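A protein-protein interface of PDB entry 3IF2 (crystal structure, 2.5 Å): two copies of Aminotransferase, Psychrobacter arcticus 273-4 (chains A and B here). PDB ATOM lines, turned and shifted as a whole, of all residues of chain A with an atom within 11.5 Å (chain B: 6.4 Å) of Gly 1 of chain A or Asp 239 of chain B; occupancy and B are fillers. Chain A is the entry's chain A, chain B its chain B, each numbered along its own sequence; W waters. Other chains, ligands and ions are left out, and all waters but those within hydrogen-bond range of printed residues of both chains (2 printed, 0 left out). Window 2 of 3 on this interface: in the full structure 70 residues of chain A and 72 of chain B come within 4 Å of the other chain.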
ATOM      1  N   GLY A   1      -5.557 -17.744  -7.135  1.00  0.00           N
ATOM      2  CA  GLY A   1      -4.105 -17.454  -6.868  1.00  0.00           C
ATOM      3  C   GLY A   1      -3.716 -16.039  -7.286  1.00  0.00           C
ATOM      4  O   GLY A   1      -4.507 -15.100  -7.117  1.00  0.00           O
ATOM      5  N   MET A   2      -2.492 -15.877  -7.790  1.00  0.00           N
ATOM      6  CA  MET A   2      -1.988 -14.594  -8.323  1.00  0.00           C
ATOM      7  C   MET A   2      -2.021 -14.711  -9.845  1.00  0.00           C
ATOM      8  O   MET A   2      -1.520 -15.700 -10.400  1.00  0.00           O
ATOM      9  CB  MET A   2      -0.531 -14.324  -7.873  1.00  0.00           C
ATOM     10  CG  MET A   2      -0.342 -13.998  -6.371  1.00  0.00           C
ATOM     11  SD  MET A   2      -0.272 -12.116  -5.889  1.00  0.00           S
ATOM     12  CE  MET A   2      -0.788 -12.347  -4.036  1.00  0.00           C
ATOM     13  N   LYS A   3      -2.618 -13.726 -10.514  1.00  0.00           N
ATOM     14  CA  LYS A   3      -2.681 -13.709 -11.978  1.00  0.00           C
ATOM     15  C   LYS A   3      -1.898 -12.496 -12.476  1.00  0.00           C
ATOM     16  O   LYS A   3      -2.131 -11.367 -12.023  1.00  0.00           O
ATOM     17  CB  LYS A   3      -4.132 -13.724 -12.442  1.00  0.00           C
ATOM     18  CG  LYS A   3      -4.784 -15.077 -12.139  1.00  0.00           C
ATOM     19  CD  LYS A   3      -6.286 -15.023 -12.053  1.00  0.00           C
ATOM     20  CE  LYS A   3      -6.849 -16.311 -11.390  1.00  0.00           C
ATOM     21  NZ  LYS A   3      -6.542 -16.394  -9.904  1.00  0.00           N
ATOM     22  N   PHE A   4      -0.951 -12.758 -13.380  1.00  0.00           N
ATOM     23  CA  PHE A   4      -0.094 -11.736 -13.944  1.00  0.00           C
ATOM     24  C   PHE A   4      -0.503 -11.301 -15.340  1.00  0.00           C
ATOM     25  O   PHE A   4      -1.187 -12.020 -16.057  1.00  0.00           O
ATOM     26  CB  PHE A   4       1.356 -12.226 -14.040  1.00  0.00           C
ATOM     27  CG  PHE A   4       1.996 -12.635 -12.732  1.00  0.00           C
ATOM     28  CD1 PHE A   4       1.642 -12.069 -11.487  1.00  0.00           C
ATOM     29  CD2 PHE A   4       3.099 -13.498 -12.775  1.00  0.00           C
ATOM     30  CE1 PHE A   4       2.313 -12.442 -10.308  1.00  0.00           C
ATOM     31  CE2 PHE A   4       3.793 -13.867 -11.600  1.00  0.00           C
ATOM     32  CZ  PHE A   4       3.391 -13.339 -10.365  1.00  0.00           C
ATOM     33  N   SER A   5      -0.017 -10.122 -15.723  1.00  0.00           N
ATOM     34  CA  SER A   5      -0.225  -9.554 -17.048  1.00  0.00           C
ATOM     35  C   SER A   5       0.649 -10.310 -18.047  1.00  0.00           C
ATOM     36  O   SER A   5       1.388 -11.219 -17.662  1.00  0.00           O
ATOM     37  CB  SER A   5       0.164  -8.074 -17.046  1.00  0.00           C
ATOM     38  OG  SER A   5       1.561  -7.906 -16.867  1.00  0.00           O
ATOM     39  N   GLN A   9       4.057 -12.361 -17.372  1.00  0.00           N
ATOM     40  CA  GLN A   9       4.232 -13.752 -17.845  1.00  0.00           C
ATOM     41  C   GLN A   9       5.545 -13.952 -18.611  1.00  0.00           C
ATOM     42  O   GLN A   9       6.084 -15.029 -18.574  1.00  0.00           O
ATOM     43  CB  GLN A   9       3.002 -14.258 -18.633  1.00  0.00           C
ATOM     44  CG  GLN A   9       1.822 -14.555 -17.729  1.00  0.00           C
ATOM     45  CD  GLN A   9       0.481 -14.801 -18.452  1.00  0.00           C
ATOM     46  OE1 GLN A   9       0.170 -14.209 -19.498  1.00  0.00           O
ATOM     47  NE2 GLN A   9      -0.342 -15.650 -17.845  1.00  0.00           N
ATOM     48  N   GLY B 208      -6.402  -5.613 -11.781  1.00  0.00           N
ATOM     49  CA  GLY B 208      -5.362  -6.600 -11.461  1.00  0.00           C
ATOM     50  C   GLY B 208      -4.685  -6.463 -10.105  1.00  0.00           C
ATOM     51  O   GLY B 208      -3.965  -7.362  -9.720  1.00  0.00           O
ATOM     52  N   ILE B 234     -11.791  -6.844   0.298  1.00  0.00           N
ATOM     53  CA  ILE B 234     -12.063  -6.578  -1.127  1.00  0.00           C
ATOM     54  C   ILE B 234     -10.984  -7.210  -2.022  1.00  0.00           C
ATOM     55  O   ILE B 234     -11.306  -7.828  -3.040  1.00  0.00           O
ATOM     56  CB  ILE B 234     -12.182  -5.062  -1.436  1.00  0.00           C
ATOM     57  CG1 ILE B 234     -13.417  -4.472  -0.764  1.00  0.00           C
ATOM     58  CG2 ILE B 234     -12.274  -4.810  -2.947  1.00  0.00           C
ATOM     59  CD1 ILE B 234     -13.556  -2.992  -0.937  1.00  0.00           C
ATOM     60  N   ALA B 235      -9.720  -7.077  -1.630  1.00  0.00           N
ATOM     61  CA  ALA B 235      -8.620  -7.670  -2.383  1.00  0.00           C
ATOM     62  C   ALA B 235      -8.770  -9.213  -2.478  1.00  0.00           C
ATOM     63  O   ALA B 235      -8.719  -9.763  -3.582  1.00  0.00           O
ATOM     64  CB  ALA B 235      -7.250  -7.264  -1.773  1.00  0.00           C
ATOM     65  N   LYS B 236      -8.992  -9.886  -1.335  1.00  0.00           N
ATOM     66  CA  LYS B 236      -9.152 -11.347  -1.303  1.00  0.00           C
ATOM     67  C   LYS B 236     -10.420 -11.784  -2.034  1.00  0.00           C
ATOM     68  O   LYS B 236     -10.394 -12.824  -2.687  1.00  0.00           O
ATOM     69  CB  LYS B 236      -9.133 -11.928   0.128  1.00  0.00           C
ATOM     70  CG  LYS B 236      -9.113 -13.478   0.165  1.00  0.00           C
ATOM     71  N   ARG B 237     -11.493 -10.988  -1.951  1.00  0.00           N
ATOM     72  CA  ARG B 237     -12.774 -11.306  -2.622  1.00  0.00           C
ATOM     73  C   ARG B 237     -12.600 -11.382  -4.136  1.00  0.00           C
ATOM     74  O   ARG B 237     -12.997 -12.372  -4.740  1.00  0.00           O
ATOM     75  CB  ARG B 237     -13.892 -10.305  -2.272  1.00  0.00           C
ATOM     76  CG  ARG B 237     -15.291 -10.756  -2.746  1.00  0.00           C
ATOM     77  CD  ARG B 237     -16.476  -9.868  -2.310  1.00  0.00           C
ATOM     78  NE  ARG B 237     -16.327  -9.412  -0.919  1.00  0.00           N
ATOM     79  CZ  ARG B 237     -16.246  -8.140  -0.485  1.00  0.00           C
ATOM     80  NH1 ARG B 237     -16.411  -7.085  -1.304  1.00  0.00           N
ATOM     81  NH2 ARG B 237     -16.060  -7.902   0.829  1.00  0.00           N
ATOM     82  N   TYR B 238     -11.976 -10.361  -4.723  1.00  0.00           N
ATOM     83  CA  TYR B 238     -11.719 -10.311  -6.175  1.00  0.00           C
ATOM     84  C   TYR B 238     -10.420 -11.007  -6.628  1.00  0.00           C
ATOM     85  O   TYR B 238     -10.037 -10.904  -7.791  1.00  0.00           O
ATOM     86  CB  TYR B 238     -11.831  -8.867  -6.685  1.00  0.00           C
ATOM     87  CG  TYR B 238     -13.237  -8.341  -6.497  1.00  0.00           C
ATOM     88  CD1 TYR B 238     -14.246  -8.621  -7.422  1.00  0.00           C
ATOM     89  CD2 TYR B 238     -13.575  -7.604  -5.367  1.00  0.00           C
ATOM     90  CE1 TYR B 238     -15.572  -8.142  -7.220  1.00  0.00           C
ATOM     91  CE2 TYR B 238     -14.860  -7.127  -5.159  1.00  0.00           C
ATOM     92  CZ  TYR B 238     -15.859  -7.394  -6.080  1.00  0.00           C
ATOM     93  OH  TYR B 238     -17.113  -6.906  -5.826  1.00  0.00           O
ATOM     94  N   ASP B 239      -9.766 -11.723  -5.714  1.00  0.00           N
ATOM     95  CA  ASP B 239      -8.585 -12.539  -5.998  1.00  0.00           C
ATOM     96  C   ASP B 239      -7.413 -11.754  -6.637  1.00  0.00           C
ATOM     97  O   ASP B 239      -6.797 -12.175  -7.634  1.00  0.00           O
ATOM     98  CB  ASP B 239      -9.040 -13.751  -6.828  1.00  0.00           C
ATOM     99  CG  ASP B 239      -8.359 -15.043  -6.406  1.00  0.00           C
ATOM    100  OD1 ASP B 239      -7.146 -15.034  -6.080  1.00  0.00           O
ATOM    101  OD2 ASP B 239      -9.076 -16.076  -6.387  1.00  0.00           O
ATOM    102  N   ILE B 240      -7.124 -10.605  -6.019  1.00  0.00           N
ATOM    103  CA  ILE B 240      -6.073  -9.666  -6.441  1.00  0.00           C
ATOM    104  C   ILE B 240      -5.281  -9.161  -5.233  1.00  0.00           C
ATOM    105  O   ILE B 240      -5.860  -8.981  -4.154  1.00  0.00           O
ATOM    106  CB  ILE B 240      -6.656  -8.447  -7.218  1.00  0.00           C
ATOM    107  CG1 ILE B 240      -7.794  -7.754  -6.439  1.00  0.00           C
ATOM    108  CG2 ILE B 240      -7.132  -8.894  -8.596  1.00  0.00           C
ATOM    109  CD1 ILE B 240      -8.231  -6.466  -7.061  1.00  0.00           C
ATOM    110  N   PRO B 241      -3.970  -8.898  -5.409  1.00  0.00           N
ATOM    111  CA  PRO B 241      -3.147  -8.466  -4.282  1.00  0.00           C
ATOM    112  C   PRO B 241      -3.382  -7.032  -3.830  1.00  0.00           C
ATOM    113  O   PRO B 241      -3.702  -6.187  -4.667  1.00  0.00           O
ATOM    114  CB  PRO B 241      -1.737  -8.569  -4.849  1.00  0.00           C
ATOM    115  CG  PRO B 241      -1.893  -8.226  -6.277  1.00  0.00           C
ATOM    116  CD  PRO B 241      -3.213  -8.820  -6.676  1.00  0.00           C
ATOM    117  N   ASN B 267      -1.459 -12.462   0.546  1.00  0.00           N
ATOM    118  CA  ASN B 267      -2.139 -11.654  -0.443  1.00  0.00           C
ATOM    119  C   ASN B 267      -1.698 -10.181  -0.393  1.00  0.00           C
ATOM    120  O   ASN B 267      -2.146  -9.408  -1.214  1.00  0.00           O
ATOM    121  CB  ASN B 267      -3.670 -11.779  -0.272  1.00  0.00           C
ATOM    122  CG  ASN B 267      -4.448 -11.389  -1.534  1.00  0.00           C
ATOM    123  OD1 ASN B 267      -4.017 -11.671  -2.660  1.00  0.00           O
ATOM    124  ND2 ASN B 267      -5.606 -10.749  -1.343  1.00  0.00           N
ATOM    125  N   LYS B 292       5.821 -16.204  -4.942  1.00  0.00           N
ATOM    126  CA  LYS B 292       5.482 -16.050  -6.357  1.00  0.00           C
ATOM    127  C   LYS B 292       5.762 -14.623  -6.881  1.00  0.00           C
ATOM    128  O   LYS B 292       6.213 -14.476  -8.012  1.00  0.00           O
ATOM    129  CB  LYS B 292       4.025 -16.538  -6.621  1.00  0.00           C
ATOM    130  CG  LYS B 292       3.676 -16.736  -8.090  1.00  0.00           C
ATOM    131  CD  LYS B 292       2.220 -17.282  -8.331  1.00  0.00           C
ATOM    132  CE  LYS B 292       1.734 -17.066  -9.792  1.00  0.00           C
ATOM    133  NZ  LYS B 292       2.757 -17.519 -10.803  1.00  0.00           N
HETATM  134  O   HOH W   1      -4.406 -11.760  -8.930  1.00  0.00           O
HETATM  135  O   HOH W   2      -4.023  -9.903 -10.725  1.00  0.00           O
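OD1 of Asp 239 of chain B lies within hydrogen-bond range of N of Gly 1 of chain A, 3.3 Å away.
The backbone carbonyl oxygen (O) of Ile 240 of chain B sits at hydrogen-bond distance from the side-chain amide nitrogen (ND2) of Asn 267 of chain B (3.3 Å).
The backbone NH of Lys 236 of chain B lies close to the side-chain amide nitrogen of Asn 267 of chain B, 3.5 Å away.
Among the printed residues, merely in contact across the chains: Met 2 of chain A with Pro 241 of chain B (3.98 Å), Met 2 of chain A with Asn 267 of chain B (3.6 Å), Met 2 of chain A with Lys 292 of chain B (3.6 Å) and Phe 4 of chain A with Lys 292 of chain B (3.8 Å).
Of the printed residues of chain B, Met 2 of chain A touches Pro 241, Asn 267 and Lys 292.
Printed residues of chain B within 4 Å of Phe 4 of chain A: Lys 292 (3.8 Å).
No residue of chain A comes within 4 Å of Ala 235 of chain B.
No residue of chain A comes within 4 Å of Lys 236 of chain B.
Asp 239 of chain B touches just one residue of chain A: Gly 1.
No residue of chain A comes within 4 Å of Ile 240 of chain B.
Pro 241 of chain B touches one residue of chain A.
Of the printed residues of chain A, Asn 267 of chain B touches Met 2 (3.6 Å).
Printed residues of chain A within 4 Å of Lys 292 of chain B: Met 2 and Phe 4.
The nearest residue of chain B that does not touch Gly 1 of chain A is Ile 240 of chain B (5.3 Å).
The nearest residue of chain A that does not touch Asp 239 of chain B is Lys 3 of chain A (4.1 Å).
The nearest printed residue of chain B that does not touch Met 2 of chain A is Asp 239 of chain B (5.0 Å).
Of the 11 printed residues of chain B, 4 touch a printed residue of chain A.
Hydrophobic or aromatic side chains of chain B within 4 Å of the printed part of chain A: Pro 241.
Among the printed residues, 5 pairs touch across the chains.
Among the printed residues, no Asp or Glu carboxylate lies within 4 Å of a Lys or Arg side-chain nitrogen of the other chain.
No position is printed for both chains.
Of the 5 pairs that touch across the chains among the printed residues, none has its exchanged pair printed and touching as well.
Water W2 lies within hydrogen-bond range of O of Lys 3 of chain A and O of Gly 208 of chain B.
Water W1 lies within hydrogen-bond range of O of Asp 239 of chain B (2.8 Å) and N of Lys 3 of chain A (3.1 Å).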
